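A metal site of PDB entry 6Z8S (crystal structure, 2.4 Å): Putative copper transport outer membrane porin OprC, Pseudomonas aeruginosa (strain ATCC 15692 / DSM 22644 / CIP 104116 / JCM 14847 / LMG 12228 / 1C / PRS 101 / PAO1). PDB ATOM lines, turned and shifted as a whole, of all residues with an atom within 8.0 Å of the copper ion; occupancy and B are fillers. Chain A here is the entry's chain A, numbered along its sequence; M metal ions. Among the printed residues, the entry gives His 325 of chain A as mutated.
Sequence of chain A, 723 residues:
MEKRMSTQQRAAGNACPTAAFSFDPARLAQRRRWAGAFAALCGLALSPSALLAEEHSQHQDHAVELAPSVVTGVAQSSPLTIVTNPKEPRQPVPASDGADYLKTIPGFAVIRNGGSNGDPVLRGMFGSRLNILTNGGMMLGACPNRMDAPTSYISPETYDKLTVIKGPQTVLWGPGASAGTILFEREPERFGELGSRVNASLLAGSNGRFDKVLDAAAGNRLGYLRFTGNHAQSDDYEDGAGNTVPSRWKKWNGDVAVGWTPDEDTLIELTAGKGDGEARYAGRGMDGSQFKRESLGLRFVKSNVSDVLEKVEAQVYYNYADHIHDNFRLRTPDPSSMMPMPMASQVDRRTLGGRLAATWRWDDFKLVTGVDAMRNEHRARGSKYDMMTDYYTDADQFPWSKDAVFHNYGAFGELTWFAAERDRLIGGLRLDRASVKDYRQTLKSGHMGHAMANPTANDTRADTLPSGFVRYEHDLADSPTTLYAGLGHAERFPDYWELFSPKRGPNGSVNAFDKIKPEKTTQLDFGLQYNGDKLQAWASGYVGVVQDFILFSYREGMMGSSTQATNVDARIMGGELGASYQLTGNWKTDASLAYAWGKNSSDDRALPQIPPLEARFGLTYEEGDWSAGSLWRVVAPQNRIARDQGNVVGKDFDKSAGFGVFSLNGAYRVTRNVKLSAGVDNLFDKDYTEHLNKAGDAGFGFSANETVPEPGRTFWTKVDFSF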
ATOM      1  N   ALA A 142       2.192 -28.552  -7.899  1.00  0.00           N
ATOM      2  CA  ALA A 142       1.486 -27.578  -8.722  1.00  0.00           C
ATOM      3  C   ALA A 142       1.706 -27.727 -10.220  1.00  0.00           C
ATOM      4  O   ALA A 142       0.964 -27.112 -10.997  1.00  0.00           O
ATOM      5  CB  ALA A 142       1.907 -26.149  -8.339  1.00  0.00           C
ATOM      6  N   CYS A 143       2.721 -28.469 -10.640  1.00  0.00           N
ATOM      7  CA  CYS A 143       3.037 -28.539 -12.065  1.00  0.00           C
ATOM      8  C   CYS A 143       1.911 -29.272 -12.796  1.00  0.00           C
ATOM      9  O   CYS A 143       1.588 -30.405 -12.443  1.00  0.00           O
ATOM     10  CB  CYS A 143       4.367 -29.243 -12.323  1.00  0.00           C
ATOM     11  SG  CYS A 143       4.760 -29.457 -14.094  1.00  0.00           S
ATOM     12  N   PRO A 144       1.312 -28.669 -13.819  1.00  0.00           N
ATOM     13  CA  PRO A 144       0.305 -29.414 -14.604  1.00  0.00           C
ATOM     14  C   PRO A 144       0.860 -30.654 -15.294  1.00  0.00           C
ATOM     15  O   PRO A 144       0.063 -31.462 -15.791  1.00  0.00           O
ATOM     16  CB  PRO A 144      -0.189 -28.362 -15.622  1.00  0.00           C
ATOM     17  CG  PRO A 144       0.867 -27.346 -15.685  1.00  0.00           C
ATOM     18  CD  PRO A 144       1.509 -27.303 -14.317  1.00  0.00           C
ATOM     19  N   ASN A 145       2.188 -30.827 -15.338  1.00  0.00           N
ATOM     20  CA  ASN A 145       2.819 -32.009 -15.913  1.00  0.00           C
ATOM     21  C   ASN A 145       3.567 -32.836 -14.869  1.00  0.00           C
ATOM     22  O   ASN A 145       4.474 -33.602 -15.218  1.00  0.00           O
ATOM     23  CB  ASN A 145       3.782 -31.601 -17.021  1.00  0.00           C
ATOM     24  CG  ASN A 145       3.071 -31.012 -18.186  1.00  0.00           C
ATOM     25  OD1 ASN A 145       2.250 -31.673 -18.819  1.00  0.00           O
ATOM     26  ND2 ASN A 145       3.350 -29.739 -18.465  1.00  0.00           N
ATOM     27  N   ARG A 146       3.246 -32.642 -13.593  1.00  0.00           N
ATOM     28  CA  ARG A 146       3.800 -33.415 -12.494  1.00  0.00           C
ATOM     29  C   ARG A 146       5.334 -33.414 -12.464  1.00  0.00           C
ATOM     30  O   ARG A 146       5.959 -34.373 -12.022  1.00  0.00           O
ATOM     31  CB  ARG A 146       3.248 -34.840 -12.516  1.00  0.00           C
ATOM     32  CG  ARG A 146       1.770 -34.921 -12.075  1.00  0.00           C
ATOM     33  CD  ARG A 146       1.282 -36.365 -11.988  1.00  0.00           C
ATOM     34  NE  ARG A 146       1.990 -37.168 -10.980  1.00  0.00           N
ATOM     35  CZ  ARG A 146       1.573 -37.301  -9.719  1.00  0.00           C
ATOM     36  NH1 ARG A 146       0.450 -36.687  -9.334  1.00  0.00           N
ATOM     37  NH2 ARG A 146       2.253 -38.041  -8.855  1.00  0.00           N
ATOM     38  N   MET A 147       5.962 -32.295 -12.850  1.00  0.00           N
ATOM     39  CA  MET A 147       7.382 -32.195 -12.548  1.00  0.00           C
ATOM     40  C   MET A 147       7.651 -32.209 -11.060  1.00  0.00           C
ATOM     41  O   MET A 147       8.807 -32.395 -10.643  1.00  0.00           O
ATOM     42  CB  MET A 147       8.027 -30.920 -13.130  1.00  0.00           C
ATOM     43  CG  MET A 147       8.107 -30.842 -14.630  1.00  0.00           C
ATOM     44  SD  MET A 147       8.618 -29.193 -15.104  1.00  0.00           S
ATOM     45  CE  MET A 147       8.368 -29.220 -16.874  1.00  0.00           C
ATOM     46  N   ASP A 148       6.635 -32.017 -10.238  1.00  0.00           N
ATOM     47  CA  ASP A 148       6.861 -31.901  -8.800  1.00  0.00           C
ATOM     48  C   ASP A 148       5.877 -32.767  -8.050  1.00  0.00           C
ATOM     49  O   ASP A 148       5.169 -32.300  -7.149  1.00  0.00           O
ATOM     50  CB  ASP A 148       6.822 -30.432  -8.340  1.00  0.00           C
ATOM     51  CG  ASP A 148       5.459 -29.762  -8.514  1.00  0.00           C
ATOM     52  OD1 ASP A 148       4.675 -30.168  -9.408  1.00  0.00           O
ATOM     53  OD2 ASP A 148       5.146 -28.826  -7.744  1.00  0.00           O
ATOM     54  N   TYR A 281      15.643 -31.518 -16.792  1.00  0.00           N
ATOM     55  CA  TYR A 281      14.808 -32.662 -17.168  1.00  0.00           C
ATOM     56  C   TYR A 281      15.141 -33.108 -18.598  1.00  0.00           C
ATOM     57  O   TYR A 281      14.711 -32.475 -19.571  1.00  0.00           O
ATOM     58  CB  TYR A 281      13.320 -32.327 -17.058  1.00  0.00           C
ATOM     59  CG  TYR A 281      12.834 -32.283 -15.637  1.00  0.00           C
ATOM     60  CD1 TYR A 281      13.203 -33.270 -14.730  1.00  0.00           C
ATOM     61  CD2 TYR A 281      12.012 -31.247 -15.194  1.00  0.00           C
ATOM     62  CE1 TYR A 281      12.764 -33.237 -13.412  1.00  0.00           C
ATOM     63  CE2 TYR A 281      11.557 -31.205 -13.868  1.00  0.00           C
ATOM     64  CZ  TYR A 281      11.932 -32.203 -12.989  1.00  0.00           C
ATOM     65  OH  TYR A 281      11.507 -32.176 -11.687  1.00  0.00           O
ATOM     66  N   ARG A 284      11.780 -33.754 -20.730  1.00  0.00           N
ATOM     67  CA  ARG A 284      10.747 -32.731 -20.856  1.00  0.00           C
ATOM     68  C   ARG A 284      11.217 -31.618 -21.788  1.00  0.00           C
ATOM     69  O   ARG A 284      12.412 -31.481 -22.067  1.00  0.00           O
ATOM     70  CB  ARG A 284      10.388 -32.089 -19.499  1.00  0.00           C
ATOM     71  CG  ARG A 284      10.181 -33.028 -18.342  1.00  0.00           C
ATOM     72  CD  ARG A 284       8.945 -33.799 -18.527  1.00  0.00           C
ATOM     73  NE  ARG A 284       8.567 -34.479 -17.297  1.00  0.00           N
ATOM     74  CZ  ARG A 284       7.435 -34.231 -16.635  1.00  0.00           C
ATOM     75  NH1 ARG A 284       6.595 -33.311 -17.107  1.00  0.00           N
ATOM     76  NH2 ARG A 284       7.167 -34.891 -15.522  1.00  0.00           N
ATOM     77  N   MET A 286      10.817 -28.522 -20.820  1.00  0.00           N
ATOM     78  CA  MET A 286      11.157 -27.453 -19.887  1.00  0.00           C
ATOM     79  C   MET A 286      11.867 -28.039 -18.676  1.00  0.00           C
ATOM     80  O   MET A 286      11.716 -29.210 -18.366  1.00  0.00           O
ATOM     81  CB  MET A 286       9.925 -26.689 -19.366  1.00  0.00           C
ATOM     82  CG  MET A 286       8.924 -26.358 -20.399  1.00  0.00           C
ATOM     83  SD  MET A 286       9.024 -24.610 -20.718  1.00  0.00           S
ATOM     84  CE  MET A 286       7.524 -24.022 -20.048  1.00  0.00           C
ATOM     85  N   ASP A 287      12.583 -27.192 -17.971  1.00  0.00           N
ATOM     86  CA  ASP A 287      13.190 -27.588 -16.718  1.00  0.00           C
ATOM     87  C   ASP A 287      12.481 -26.914 -15.552  1.00  0.00           C
ATOM     88  O   ASP A 287      11.778 -25.920 -15.722  1.00  0.00           O
ATOM     89  CB  ASP A 287      14.683 -27.243 -16.690  1.00  0.00           C
ATOM     90  CG  ASP A 287      15.395 -27.699 -17.948  1.00  0.00           C
ATOM     91  OD1 ASP A 287      15.528 -28.939 -18.157  1.00  0.00           O
ATOM     92  OD2 ASP A 287      15.752 -26.809 -18.742  1.00  0.00           O
ATOM     93  N   GLY A 288      12.681 -27.500 -14.376  1.00  0.00           N
ATOM     94  CA  GLY A 288      12.152 -26.996 -13.142  1.00  0.00           C
ATOM     95  C   GLY A 288      13.174 -26.065 -12.518  1.00  0.00           C
ATOM     96  O   GLY A 288      14.172 -26.520 -11.948  1.00  0.00           O
ATOM     97  N   SER A 289      12.929 -24.762 -12.632  1.00  0.00           N
ATOM     98  CA  SER A 289      13.838 -23.806 -12.038  1.00  0.00           C
ATOM     99  C   SER A 289      13.456 -23.411 -10.617  1.00  0.00           C
ATOM    100  O   SER A 289      14.249 -22.737  -9.951  1.00  0.00           O
ATOM    101  CB  SER A 289      13.953 -22.566 -12.949  1.00  0.00           C
ATOM    102  OG  SER A 289      12.759 -21.809 -12.932  1.00  0.00           O
ATOM    103  N   GLN A 290      12.303 -23.843 -10.099  1.00  0.00           N
ATOM    104  CA  GLN A 290      11.978 -23.557  -8.710  1.00  0.00           C
ATOM    105  C   GLN A 290      10.973 -24.582  -8.202  1.00  0.00           C
ATOM    106  O   GLN A 290      10.037 -24.970  -8.901  1.00  0.00           O
ATOM    107  CB  GLN A 290      11.433 -22.120  -8.561  1.00  0.00           C
ATOM    108  CG  GLN A 290      10.961 -21.767  -7.168  1.00  0.00           C
ATOM    109  CD  GLN A 290      10.289 -20.407  -7.106  1.00  0.00           C
ATOM    110  OE1 GLN A 290      10.962 -19.393  -7.093  1.00  0.00           O
ATOM    111  NE2 GLN A 290       8.947 -20.392  -7.097  1.00  0.00           N
ATOM    112  N   PHE A 291      11.178 -25.022  -6.961  1.00  0.00           N
ATOM    113  CA  PHE A 291      10.281 -25.952  -6.266  1.00  0.00           C
ATOM    114  C   PHE A 291      10.133 -25.452  -4.836  1.00  0.00           C
ATOM    115  O   PHE A 291      10.596 -26.089  -3.894  1.00  0.00           O
ATOM    116  CB  PHE A 291      10.822 -27.387  -6.238  1.00  0.00           C
ATOM    117  CG  PHE A 291      10.958 -28.035  -7.579  1.00  0.00           C
ATOM    118  CD1 PHE A 291      12.016 -27.732  -8.398  1.00  0.00           C
ATOM    119  CD2 PHE A 291      10.045 -28.988  -7.995  1.00  0.00           C
ATOM    120  CE1 PHE A 291      12.150 -28.329  -9.621  1.00  0.00           C
ATOM    121  CE2 PHE A 291      10.169 -29.605  -9.212  1.00  0.00           C
ATOM    122  CZ  PHE A 291      11.229 -29.278 -10.033  1.00  0.00           C
ATOM    123  N   HIS A 323       5.942 -23.456  -7.913  1.00  0.00           N
ATOM    124  CA  HIS A 323       6.783 -24.096  -8.921  1.00  0.00           C
ATOM    125  C   HIS A 323       6.935 -23.225 -10.157  1.00  0.00           C
ATOM    126  O   HIS A 323       5.995 -22.554 -10.593  1.00  0.00           O
ATOM    127  CB  HIS A 323       6.174 -25.454  -9.289  1.00  0.00           C
ATOM    128  CG  HIS A 323       6.877 -26.135 -10.401  1.00  0.00           C
ATOM    129  ND1 HIS A 323       8.226 -26.404 -10.356  1.00  0.00           N
ATOM    130  CD2 HIS A 323       6.453 -26.557 -11.614  1.00  0.00           C
ATOM    131  CE1 HIS A 323       8.590 -26.987 -11.484  1.00  0.00           C
ATOM    132  NE2 HIS A 323       7.539 -27.075 -12.260  1.00  0.00           N
ATOM    133  N   ILE A 324       8.132 -23.225 -10.740  1.00  0.00           N
ATOM    134  CA  ILE A 324       8.377 -22.564 -12.012  1.00  0.00           C
ATOM    135  C   ILE A 324       9.080 -23.546 -12.943  1.00  0.00           C
ATOM    136  O   ILE A 324      10.025 -24.238 -12.550  1.00  0.00           O
ATOM    137  CB  ILE A 324       9.235 -21.304 -11.849  1.00  0.00           C
ATOM    138  CG1 ILE A 324       8.612 -20.333 -10.841  1.00  0.00           C
ATOM    139  CG2 ILE A 324       9.432 -20.614 -13.208  1.00  0.00           C
ATOM    140  CD1 ILE A 324       9.497 -19.151 -10.517  1.00  0.00           C
ATOM    141  N   HIS A 325       8.625 -23.600 -14.195  1.00  0.00           N
ATOM    142  CA  HIS A 325       9.373 -24.293 -15.224  1.00  0.00           C
ATOM    143  C   HIS A 325       9.573 -23.343 -16.407  1.00  0.00           C
ATOM    144  O   HIS A 325       8.765 -22.437 -16.630  1.00  0.00           O
ATOM    145  CB  HIS A 325       8.686 -25.616 -15.614  1.00  0.00           C
ATOM    146  CG  HIS A 325       7.311 -25.465 -16.181  1.00  0.00           C
ATOM    147  ND1 HIS A 325       6.267 -26.291 -15.828  1.00  0.00           N
ATOM    148  CD2 HIS A 325       6.825 -24.625 -17.117  1.00  0.00           C
ATOM    149  CE1 HIS A 325       5.186 -25.964 -16.516  1.00  0.00           C
ATOM    150  NE2 HIS A 325       5.502 -24.957 -17.310  1.00  0.00           N
ATOM    151  N   ASP A 326      10.681 -23.525 -17.127  1.00  0.00           N
ATOM    152  CA  ASP A 326      11.006 -22.612 -18.211  1.00  0.00           C
ATOM    153  C   ASP A 326      12.006 -23.283 -19.136  1.00  0.00           C
ATOM    154  O   ASP A 326      12.506 -24.379 -18.860  1.00  0.00           O
ATOM    155  CB  ASP A 326      11.544 -21.294 -17.700  1.00  0.00           C
ATOM    156  CG  ASP A 326      12.856 -21.447 -16.967  1.00  0.00           C
ATOM    157  OD1 ASP A 326      13.901 -21.697 -17.621  1.00  0.00           O
ATOM    158  OD2 ASP A 326      12.851 -21.312 -15.720  1.00  0.00           O
ATOM    159  N   SER A 345       6.478 -20.531 -17.006  1.00  0.00           N
ATOM    160  CA  SER A 345       5.169 -20.634 -16.392  1.00  0.00           C
ATOM    161  C   SER A 345       5.346 -20.846 -14.893  1.00  0.00           C
ATOM    162  O   SER A 345       6.245 -21.574 -14.470  1.00  0.00           O
ATOM    163  CB  SER A 345       4.375 -21.774 -17.039  1.00  0.00           C
ATOM    164  OG  SER A 345       3.222 -22.055 -16.288  1.00  0.00           O
ATOM    165  N   GLN A 346       4.518 -20.171 -14.094  1.00  0.00           N
ATOM    166  CA  GLN A 346       4.589 -20.261 -12.633  1.00  0.00           C
ATOM    167  C   GLN A 346       3.256 -20.729 -12.099  1.00  0.00           C
ATOM    168  O   GLN A 346       2.202 -20.161 -12.427  1.00  0.00           O
ATOM    169  CB  GLN A 346       4.936 -18.925 -11.984  1.00  0.00           C
ATOM    170  CG  GLN A 346       5.025 -19.018 -10.452  1.00  0.00           C
ATOM    171  CD  GLN A 346       5.547 -17.761  -9.786  1.00  0.00           C
ATOM    172  OE1 GLN A 346       5.462 -16.668 -10.334  1.00  0.00           O
ATOM    173  NE2 GLN A 346       6.091 -17.910  -8.589  1.00  0.00           N
ATOM    174  N   VAL A 347       3.288 -21.749 -11.248  1.00  0.00           N
ATOM    175  CA  VAL A 347       2.077 -22.350 -10.738  1.00  0.00           C
ATOM    176  C   VAL A 347       2.268 -22.606  -9.259  1.00  0.00           C
ATOM    177  O   VAL A 347       3.388 -22.827  -8.792  1.00  0.00           O
ATOM    178  CB  VAL A 347       1.757 -23.657 -11.503  1.00  0.00           C
ATOM    179  CG1 VAL A 347       1.311 -23.339 -12.877  1.00  0.00           C
ATOM    180  CG2 VAL A 347       2.973 -24.580 -11.523  1.00  0.00           C
HETATM  181 CU    CU M   1       6.656 -27.830 -14.228  1.00  0.00          CU
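Within 4 Å of the copper ion: Cys 143, Met 147, His 323 and His 325.
The copper ion is bound by ND1 of His 325, NE2 of His 323, SG of Cys 143 and SD of Met 147. The copper ion has four donor atoms within binding distance.
O of His 325 is in hydrogen-bond range of N of Ser 345. The backbone carbonyl oxygen of Val 347 is in hydrogen-bond range of the backbone NH of His 323, at 2.8 Å. O of Gln 290 is in hydrogen-bond range of ND1 of His 323 (2.7 Å). N of Asn 145 sits close to SG of Cys 143 (3.2 Å). The side-chain carboxylate (OD1) of Asp 148 lies within hydrogen-bond range of the backbone NH (N) of Cys 143, 2.9 Å away. SG of Cys 143 lies close to N of Arg 146 (3.6 Å). O of Met 147 is in hydrogen-bond range of OH of Tyr 281 (2.9 Å).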
